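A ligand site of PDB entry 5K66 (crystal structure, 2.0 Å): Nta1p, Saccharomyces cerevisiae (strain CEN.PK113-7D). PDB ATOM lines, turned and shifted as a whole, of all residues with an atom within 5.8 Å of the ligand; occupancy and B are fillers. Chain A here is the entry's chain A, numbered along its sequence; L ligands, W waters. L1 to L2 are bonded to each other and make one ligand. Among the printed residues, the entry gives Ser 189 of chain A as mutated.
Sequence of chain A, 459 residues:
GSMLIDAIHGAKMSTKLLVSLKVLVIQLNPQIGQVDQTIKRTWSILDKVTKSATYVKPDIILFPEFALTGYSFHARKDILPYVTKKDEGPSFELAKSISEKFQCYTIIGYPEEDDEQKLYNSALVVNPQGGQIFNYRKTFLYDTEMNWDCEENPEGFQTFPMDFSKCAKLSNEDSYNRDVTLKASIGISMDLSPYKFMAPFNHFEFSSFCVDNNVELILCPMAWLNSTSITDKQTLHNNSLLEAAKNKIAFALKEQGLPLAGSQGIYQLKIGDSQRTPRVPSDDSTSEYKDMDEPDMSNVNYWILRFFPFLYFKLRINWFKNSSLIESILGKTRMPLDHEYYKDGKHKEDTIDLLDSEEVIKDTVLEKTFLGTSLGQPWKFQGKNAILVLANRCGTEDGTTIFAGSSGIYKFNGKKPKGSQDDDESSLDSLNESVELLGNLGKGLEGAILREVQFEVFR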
ATOM      1  N   GLU A  65       9.899 -10.645  -1.804  1.00  0.00           N
ATOM      2  CA  GLU A  65       9.258  -9.334  -1.923  1.00  0.00           C
ATOM      3  C   GLU A  65       8.644  -8.939  -0.596  1.00  0.00           C
ATOM      4  O   GLU A  65       7.995  -9.764   0.048  1.00  0.00           O
ATOM      5  CB  GLU A  65       8.197  -9.370  -3.051  1.00  0.00           C
ATOM      6  CG  GLU A  65       7.312  -8.114  -3.210  1.00  0.00           C
ATOM      7  CD  GLU A  65       6.449  -8.182  -4.474  1.00  0.00           C
ATOM      8  OE1 GLU A  65       6.329  -9.290  -5.049  1.00  0.00           O
ATOM      9  OE2 GLU A  65       5.893  -7.150  -4.902  1.00  0.00           O
ATOM     10  N   TYR A  71       2.534  -8.058   2.826  1.00  0.00           N
ATOM     11  CA  TYR A  71       2.372  -7.623   1.437  1.00  0.00           C
ATOM     12  C   TYR A  71       1.078  -6.865   1.138  1.00  0.00           C
ATOM     13  O   TYR A  71       1.103  -5.863   0.429  1.00  0.00           O
ATOM     14  CB  TYR A  71       2.466  -8.827   0.494  1.00  0.00           C
ATOM     15  CG  TYR A  71       2.346  -8.429  -0.966  1.00  0.00           C
ATOM     16  CD1 TYR A  71       3.360  -7.714  -1.591  1.00  0.00           C
ATOM     17  CD2 TYR A  71       1.193  -8.703  -1.702  1.00  0.00           C
ATOM     18  CE1 TYR A  71       3.256  -7.303  -2.899  1.00  0.00           C
ATOM     19  CE2 TYR A  71       1.079  -8.307  -3.020  1.00  0.00           C
ATOM     20  CZ  TYR A  71       2.106  -7.610  -3.609  1.00  0.00           C
ATOM     21  OH  TYR A  71       1.989  -7.203  -4.920  1.00  0.00           O
ATOM     22  N   LYS A 138      10.313  -2.162  -8.389  1.00  0.00           N
ATOM     23  CA  LYS A 138       9.420  -2.994  -9.195  1.00  0.00           C
ATOM     24  C   LYS A 138       8.944  -2.196 -10.415  1.00  0.00           C
ATOM     25  O   LYS A 138       8.645  -0.994 -10.323  1.00  0.00           O
ATOM     26  CB  LYS A 138       8.229  -3.473  -8.349  1.00  0.00           C
ATOM     27  CG  LYS A 138       7.405  -4.591  -8.958  1.00  0.00           C
ATOM     28  CD  LYS A 138       6.292  -4.984  -7.948  1.00  0.00           C
ATOM     29  CE  LYS A 138       5.525  -6.225  -8.432  1.00  0.00           C
ATOM     30  NZ  LYS A 138       4.631  -6.732  -7.349  1.00  0.00           N
ATOM     31  N   PHE A 140       6.775  -3.682 -13.277  1.00  0.00           N
ATOM     32  CA  PHE A 140       5.366  -3.984 -13.584  1.00  0.00           C
ATOM     33  C   PHE A 140       4.607  -4.117 -12.268  1.00  0.00           C
ATOM     34  O   PHE A 140       4.921  -4.999 -11.462  1.00  0.00           O
ATOM     35  CB  PHE A 140       5.233  -5.293 -14.384  1.00  0.00           C
ATOM     36  CG  PHE A 140       5.716  -5.190 -15.808  1.00  0.00           C
ATOM     37  CD1 PHE A 140       6.174  -3.996 -16.337  1.00  0.00           C
ATOM     38  CD2 PHE A 140       5.704  -6.308 -16.626  1.00  0.00           C
ATOM     39  CE1 PHE A 140       6.626  -3.923 -17.663  1.00  0.00           C
ATOM     40  CE2 PHE A 140       6.128  -6.247 -17.948  1.00  0.00           C
ATOM     41  CZ  PHE A 140       6.591  -5.045 -18.472  1.00  0.00           C
ATOM     42  N   LEU A 141       3.602  -3.275 -12.030  1.00  0.00           N
ATOM     43  CA  LEU A 141       2.928  -3.314 -10.736  1.00  0.00           C
ATOM     44  C   LEU A 141       1.718  -4.254 -10.760  1.00  0.00           C
ATOM     45  O   LEU A 141       1.072  -4.444 -11.789  1.00  0.00           O
ATOM     46  CB  LEU A 141       2.470  -1.923 -10.287  1.00  0.00           C
ATOM     47  CG  LEU A 141       3.533  -0.817 -10.217  1.00  0.00           C
ATOM     48  CD1 LEU A 141       2.953   0.445  -9.616  1.00  0.00           C
ATOM     49  CD2 LEU A 141       4.790  -1.283  -9.469  1.00  0.00           C
ATOM     50  N   TYR A 142       1.440  -4.820  -9.595  1.00  0.00           N
ATOM     51  CA  TYR A 142       0.287  -5.681  -9.400  1.00  0.00           C
ATOM     52  C   TYR A 142      -0.852  -4.844  -8.788  1.00  0.00           C
ATOM     53  O   TYR A 142      -0.635  -3.744  -8.299  1.00  0.00           O
ATOM     54  CB  TYR A 142       0.681  -6.865  -8.490  1.00  0.00           C
ATOM     55  CG  TYR A 142      -0.411  -7.861  -8.216  1.00  0.00           C
ATOM     56  CD1 TYR A 142      -1.031  -8.555  -9.260  1.00  0.00           C
ATOM     57  CD2 TYR A 142      -0.807  -8.141  -6.904  1.00  0.00           C
ATOM     58  CE1 TYR A 142      -2.048  -9.483  -8.999  1.00  0.00           C
ATOM     59  CE2 TYR A 142      -1.802  -9.076  -6.635  1.00  0.00           C
ATOM     60  CZ  TYR A 142      -2.420  -9.735  -7.693  1.00  0.00           C
ATOM     61  OH  TYR A 142      -3.413 -10.645  -7.420  1.00  0.00           O
ATOM     62  N   ASP A 143      -2.071  -5.372  -8.820  1.00  0.00           N
ATOM     63  CA  ASP A 143      -3.241  -4.688  -8.259  1.00  0.00           C
ATOM     64  C   ASP A 143      -3.006  -4.148  -6.857  1.00  0.00           C
ATOM     65  O   ASP A 143      -3.376  -3.013  -6.548  1.00  0.00           O
ATOM     66  CB  ASP A 143      -4.429  -5.639  -8.266  1.00  0.00           C
ATOM     67  CG  ASP A 143      -4.779  -6.132  -9.664  1.00  0.00           C
ATOM     68  OD1 ASP A 143      -3.845  -6.490 -10.436  1.00  0.00           O
ATOM     69  OD2 ASP A 143      -5.988  -6.126  -9.994  1.00  0.00           O
ATOM     70  N   GLU A 145      -0.277  -3.082  -5.351  1.00  0.00           N
ATOM     71  CA  GLU A 145       0.513  -1.849  -5.361  1.00  0.00           C
ATOM     72  C   GLU A 145      -0.312  -0.606  -5.646  1.00  0.00           C
ATOM     73  O   GLU A 145       0.006   0.474  -5.168  1.00  0.00           O
ATOM     74  CB  GLU A 145       1.642  -1.904  -6.397  1.00  0.00           C
ATOM     75  CG  GLU A 145       2.906  -2.544  -5.892  1.00  0.00           C
ATOM     76  CD  GLU A 145       2.861  -4.038  -6.001  1.00  0.00           C
ATOM     77  OE1 GLU A 145       2.729  -4.546  -7.141  1.00  0.00           O
ATOM     78  OE2 GLU A 145       2.984  -4.709  -4.944  1.00  0.00           O
ATOM     79  N   ILE A 188      11.055  -8.317  -9.672  1.00  0.00           N
ATOM     80  CA  ILE A 188      10.146  -8.524  -8.549  1.00  0.00           C
ATOM     81  C   ILE A 188       8.792  -9.010  -9.070  1.00  0.00           C
ATOM     82  O   ILE A 188       8.141  -8.311  -9.858  1.00  0.00           O
ATOM     83  CB  ILE A 188       9.997  -7.220  -7.722  1.00  0.00           C
ATOM     84  CG1 ILE A 188      11.358  -6.784  -7.175  1.00  0.00           C
ATOM     85  CG2 ILE A 188       9.009  -7.413  -6.581  1.00  0.00           C
ATOM     86  CD1 ILE A 188      11.341  -5.408  -6.488  1.00  0.00           C
ATOM     87  N   SER A 189       8.421 -10.217  -8.654  1.00  0.00           N
ATOM     88  CA  SER A 189       7.161 -10.916  -9.012  1.00  0.00           C
ATOM     89  C   SER A 189       6.466 -10.495 -10.314  1.00  0.00           C
ATOM     90  O   SER A 189       6.758 -11.060 -11.364  1.00  0.00           O
ATOM     91  CB  SER A 189       6.153 -10.799  -7.861  1.00  0.00           C
ATOM     92  OG  SER A 189       5.815  -9.452  -7.594  1.00  0.00           O
ATOM     93  N   MET A 190       5.523  -9.549 -10.234  1.00  0.00           N
ATOM     94  CA  MET A 190       4.786  -9.113 -11.432  1.00  0.00           C
ATOM     95  C   MET A 190       5.672  -8.715 -12.633  1.00  0.00           C
ATOM     96  O   MET A 190       5.201  -8.697 -13.762  1.00  0.00           O
ATOM     97  CB  MET A 190       3.872  -7.937 -11.084  1.00  0.00           C
ATOM     98  CG  MET A 190       2.961  -7.487 -12.228  1.00  0.00           C
ATOM     99  SD  MET A 190       1.522  -8.576 -12.437  1.00  0.00           S
ATOM    100  CE  MET A 190       0.817  -7.941 -13.970  1.00  0.00           C
ATOM    101  N   SER A 193       5.310 -11.124 -15.412  1.00  0.00           N
ATOM    102  CA  SER A 193       4.004 -11.266 -16.066  1.00  0.00           C
ATOM    103  C   SER A 193       3.908 -10.382 -17.306  1.00  0.00           C
ATOM    104  O   SER A 193       4.698  -9.461 -17.469  1.00  0.00           O
ATOM    105  CB  SER A 193       2.873 -10.891 -15.096  1.00  0.00           C
ATOM    106  OG  SER A 193       2.957 -11.650 -13.906  1.00  0.00           O
ATOM    107  N   PHE A 197      -1.119  -7.584 -17.089  1.00  0.00           N
ATOM    108  CA  PHE A 197      -1.920  -8.740 -17.518  1.00  0.00           C
ATOM    109  C   PHE A 197      -2.703  -8.461 -18.806  1.00  0.00           C
ATOM    110  O   PHE A 197      -3.666  -9.157 -19.097  1.00  0.00           O
ATOM    111  CB  PHE A 197      -2.913  -9.168 -16.433  1.00  0.00           C
ATOM    112  CG  PHE A 197      -2.286  -9.658 -15.166  1.00  0.00           C
ATOM    113  CD1 PHE A 197      -1.407 -10.750 -15.187  1.00  0.00           C
ATOM    114  CD2 PHE A 197      -2.586  -9.043 -13.953  1.00  0.00           C
ATOM    115  CE1 PHE A 197      -0.833 -11.204 -14.004  1.00  0.00           C
ATOM    116  CE2 PHE A 197      -2.003  -9.502 -12.773  1.00  0.00           C
ATOM    117  CZ  PHE A 197      -1.133 -10.584 -12.799  1.00  0.00           C
ATOM    118  N   MET A 222       9.725 -12.449  -4.629  1.00  0.00           N
ATOM    119  CA  MET A 222       8.314 -12.509  -5.029  1.00  0.00           C
ATOM    120  C   MET A 222       7.328 -12.659  -3.872  1.00  0.00           C
ATOM    121  O   MET A 222       7.693 -13.141  -2.807  1.00  0.00           O
ATOM    122  CB  MET A 222       8.073 -13.690  -5.975  1.00  0.00           C
ATOM    123  CG  MET A 222       8.833 -13.715  -7.262  1.00  0.00           C
ATOM    124  SD  MET A 222       8.160 -15.124  -8.210  1.00  0.00           S
ATOM    125  CE  MET A 222       9.054 -14.922  -9.728  1.00  0.00           C
ATOM    126  N   ALA A 223       6.079 -12.248  -4.108  1.00  0.00           N
ATOM    127  CA  ALA A 223       4.968 -12.559  -3.224  1.00  0.00           C
ATOM    128  C   ALA A 223       3.876 -13.063  -4.155  1.00  0.00           C
ATOM    129  O   ALA A 223       2.920 -12.350  -4.440  1.00  0.00           O
ATOM    130  CB  ALA A 223       4.515 -11.346  -2.426  1.00  0.00           C
ATOM    131  N   TRP A 224       4.092 -14.268  -4.679  1.00  0.00           N
ATOM    132  CA  TRP A 224       3.332 -14.796  -5.810  1.00  0.00           C
ATOM    133  C   TRP A 224       2.246 -15.748  -5.315  1.00  0.00           C
ATOM    134  O   TRP A 224       2.521 -16.607  -4.484  1.00  0.00           O
ATOM    135  CB  TRP A 224       4.276 -15.519  -6.769  1.00  0.00           C
ATOM    136  CG  TRP A 224       3.647 -15.882  -8.077  1.00  0.00           C
ATOM    137  CD1 TRP A 224       2.779 -16.910  -8.318  1.00  0.00           C
ATOM    138  CD2 TRP A 224       3.862 -15.223  -9.337  1.00  0.00           C
ATOM    139  NE1 TRP A 224       2.429 -16.926  -9.645  1.00  0.00           N
ATOM    140  CE2 TRP A 224       3.087 -15.910 -10.297  1.00  0.00           C
ATOM    141  CE3 TRP A 224       4.643 -14.142  -9.755  1.00  0.00           C
ATOM    142  CZ2 TRP A 224       3.039 -15.525 -11.645  1.00  0.00           C
ATOM    143  CZ3 TRP A 224       4.609 -13.760 -11.092  1.00  0.00           C
ATOM    144  CH2 TRP A 224       3.825 -14.458 -12.023  1.00  0.00           C
ATOM    145  N   LEU A 225       1.042 -15.588  -5.844  1.00  0.00           N
ATOM    146  CA  LEU A 225      -0.149 -16.305  -5.390  1.00  0.00           C
ATOM    147  C   LEU A 225      -0.290 -17.754  -5.865  1.00  0.00           C
ATOM    148  O   LEU A 225      -0.041 -18.081  -7.024  1.00  0.00           O
ATOM    149  CB  LEU A 225      -1.411 -15.560  -5.827  1.00  0.00           C
ATOM    150  CG  LEU A 225      -1.931 -14.461  -4.913  1.00  0.00           C
ATOM    151  CD1 LEU A 225      -0.849 -13.445  -4.664  1.00  0.00           C
ATOM    152  CD2 LEU A 225      -3.200 -13.817  -5.523  1.00  0.00           C
ATOM    153  N   THR A 231      -9.238 -14.181  -6.464  1.00  0.00           N
ATOM    154  CA  THR A 231      -8.800 -13.050  -7.272  1.00  0.00           C
ATOM    155  C   THR A 231      -9.905 -12.515  -8.199  1.00  0.00           C
ATOM    156  O   THR A 231      -9.736 -11.452  -8.795  1.00  0.00           O
ATOM    157  CB  THR A 231      -7.563 -13.395  -8.125  1.00  0.00           C
ATOM    158  OG1 THR A 231      -7.849 -14.541  -8.931  1.00  0.00           O
ATOM    159  CG2 THR A 231      -6.344 -13.706  -7.218  1.00  0.00           C
ATOM    160  N   ASN A 299       2.698 -23.495 -10.169  1.00  0.00           N
ATOM    161  CA  ASN A 299       3.444 -22.241 -10.248  1.00  0.00           C
ATOM    162  C   ASN A 299       4.875 -22.421 -10.717  1.00  0.00           C
ATOM    163  O   ASN A 299       5.393 -21.581 -11.437  1.00  0.00           O
ATOM    164  CB  ASN A 299       3.424 -21.535  -8.899  1.00  0.00           C
ATOM    165  CG  ASN A 299       2.237 -20.615  -8.781  1.00  0.00           C
ATOM    166  OD1 ASN A 299       1.870 -19.937  -9.744  1.00  0.00           O
ATOM    167  ND2 ASN A 299       1.595 -20.621  -7.631  1.00  0.00           N
ATOM    168  N   TYR A 302       4.709 -22.588 -14.341  1.00  0.00           N
ATOM    169  CA  TYR A 302       4.351 -21.317 -14.919  1.00  0.00           C
ATOM    170  C   TYR A 302       5.543 -20.369 -14.890  1.00  0.00           C
ATOM    171  O   TYR A 302       5.799 -19.683 -15.859  1.00  0.00           O
ATOM    172  CB  TYR A 302       3.167 -20.690 -14.193  1.00  0.00           C
ATOM    173  CG  TYR A 302       2.730 -19.377 -14.795  1.00  0.00           C
ATOM    174  CD1 TYR A 302       1.893 -19.341 -15.908  1.00  0.00           C
ATOM    175  CD2 TYR A 302       3.159 -18.171 -14.268  1.00  0.00           C
ATOM    176  CE1 TYR A 302       1.496 -18.131 -16.479  1.00  0.00           C
ATOM    177  CE2 TYR A 302       2.759 -16.954 -14.824  1.00  0.00           C
ATOM    178  CZ  TYR A 302       1.933 -16.950 -15.922  1.00  0.00           C
ATOM    179  OH  TYR A 302       1.533 -15.739 -16.469  1.00  0.00           O
ATOM    180  N   PHE A 403      -0.204 -17.329  -0.588  1.00  0.00           N
ATOM    181  CA  PHE A 403       1.043 -17.254  -1.359  1.00  0.00           C
ATOM    182  C   PHE A 403       1.580 -18.646  -1.617  1.00  0.00           C
ATOM    183  O   PHE A 403       1.364 -19.552  -0.813  1.00  0.00           O
ATOM    184  CB  PHE A 403       2.057 -16.394  -0.616  1.00  0.00           C
ATOM    185  CG  PHE A 403       1.588 -14.970  -0.456  1.00  0.00           C
ATOM    186  CD1 PHE A 403       1.674 -14.078  -1.521  1.00  0.00           C
ATOM    187  CD2 PHE A 403       1.036 -14.533   0.744  1.00  0.00           C
ATOM    188  CE1 PHE A 403       1.224 -12.776  -1.404  1.00  0.00           C
ATOM    189  CE2 PHE A 403       0.597 -13.212   0.862  1.00  0.00           C
ATOM    190  CZ  PHE A 403       0.695 -12.336  -0.213  1.00  0.00           C
HETATM  191  N1  LIG L   1       2.267 -11.227  -9.979  1.00  0.00           N
HETATM  192  C1  LIG L   1       2.061 -11.906  -8.695  1.00  0.00           C
HETATM  193  C2  LIG L   1       1.063 -13.056  -8.827  1.00  0.00           C
HETATM  194  O1  LIG L   1       0.761 -13.763  -7.862  1.00  0.00           O
HETATM  195  C3  LIG L   1       1.590 -10.916  -7.625  1.00  0.00           C
HETATM  196  C4  LIG L   1       2.644  -9.878  -7.278  1.00  0.00           C
HETATM  197  O2  LIG L   1       2.983  -9.017  -8.096  1.00  0.00           O
HETATM  198  N2  LIG L   1       3.163  -9.951  -6.052  1.00  0.00           N
HETATM  199  N1  LG2 L   2       0.530 -13.233 -10.036  1.00  0.00           N
HETATM  200  C1  LG2 L   2      -0.314 -14.395 -10.327  1.00  0.00           C
HETATM  201  C2  LG2 L   2      -0.320 -14.709 -11.828  1.00  0.00           C
HETATM  202  O1  LG2 L   2      -0.467 -15.864 -12.221  1.00  0.00           O
HETATM  203  C3  LG2 L   2      -1.746 -14.172  -9.819  1.00  0.00           C
HETATM  204  C4  LG2 L   2      -2.412 -12.906 -10.301  1.00  0.00           C
HETATM  205  C5  LG2 L   2      -3.921 -12.886 -10.033  1.00  0.00           C
HETATM  206  O2  LG2 L   2      -4.605 -13.864 -10.393  1.00  0.00           O
HETATM  207  O3  LG2 L   2      -4.407 -11.889  -9.458  1.00  0.00           O
HETATM  208  O   HOH W   1      -4.219 -16.969  -9.235  1.00  0.00           O
HETATM  209  O   HOH W   2      -0.101 -18.605 -12.281  1.00  0.00           O
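The backbone carbonyl oxygen (O) of Ala 223 lies within hydrogen-bond range of a nitrogen (N2) of LIG L1, at 2.9 Å.
N1 of LIG L1 lies close to SD of Met 190 (3.7 Å).
OH of Tyr 71 sits at hydrogen-bond distance from N2 of LIG L1 (3.2 Å).
NZ of Lys 138 lies within hydrogen-bond range of O2 of LIG L1, 2.9 Å away.
O1 of LIG L1 lies within hydrogen-bond range of N of Leu 225, 2.7 Å away.
OE1 of Glu 65 sits at hydrogen-bond distance from N2 of LIG L1 (3.4 Å).
The side-chain hydroxyl (OH) of Tyr 142 lies within hydrogen-bond range of an oxygen (O3) of LG2 L2, 2.6 Å away.
An oxygen (O2) of LIG L1 lies within hydrogen-bond range of the side-chain hydroxyl (OG) of Ser 189 (2.9 Å).
An oxygen (O2) of LIG L1 sits close to the backbone NH of Met 190.
The backbone carbonyl oxygen (O) of Leu 225 sits at hydrogen-bond distance from the side-chain amide nitrogen (ND2) of Asn 299, at 3.1 Å.
The side-chain carboxylate (OE1) of Glu 65 lies within hydrogen-bond range of the backbone NH (N) of Ala 223 (3.1 Å).
The side-chain carboxylate (OE1) of Glu 145 lies within hydrogen-bond range of the backbone NH (N) of Tyr 142 (2.8 Å).
OD1 of Asn 299 sits at hydrogen-bond distance from NE1 of Trp 224 (3.1 Å).
The side-chain carboxylate (OE2) of Glu 65 lies within salt-bridge range of the side-chain amino group (NZ) of Lys 138 (2.8 Å).
OH of Tyr 71 sits at hydrogen-bond distance from OE2 of Glu 145 (2.7 Å).
The backbone NH (N) of Glu 65 lies within hydrogen-bond range of the backbone carbonyl oxygen (O) of Met 222 (3.5 Å).
OG of Ser 189 lies within hydrogen-bond range of OE1 of Glu 65 (2.6 Å).
Residues that only touch the ligand: Phe 197, Trp 224 and Thr 231.
Within 4 Å of the ligand: Glu 65, Tyr 71, Lys 138, Tyr 142, Ser 189, Met 190, Phe 197, Ala 223, Trp 224, Leu 225 and Thr 231.
The nearest printed residue that does not touch the ligand is Ser 193 (4.01 Å).
Water W2 lies within hydrogen-bond range of O1 of LG2 L2 (2.8 Å) and OD1 of Asn 299 (3.5 Å).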
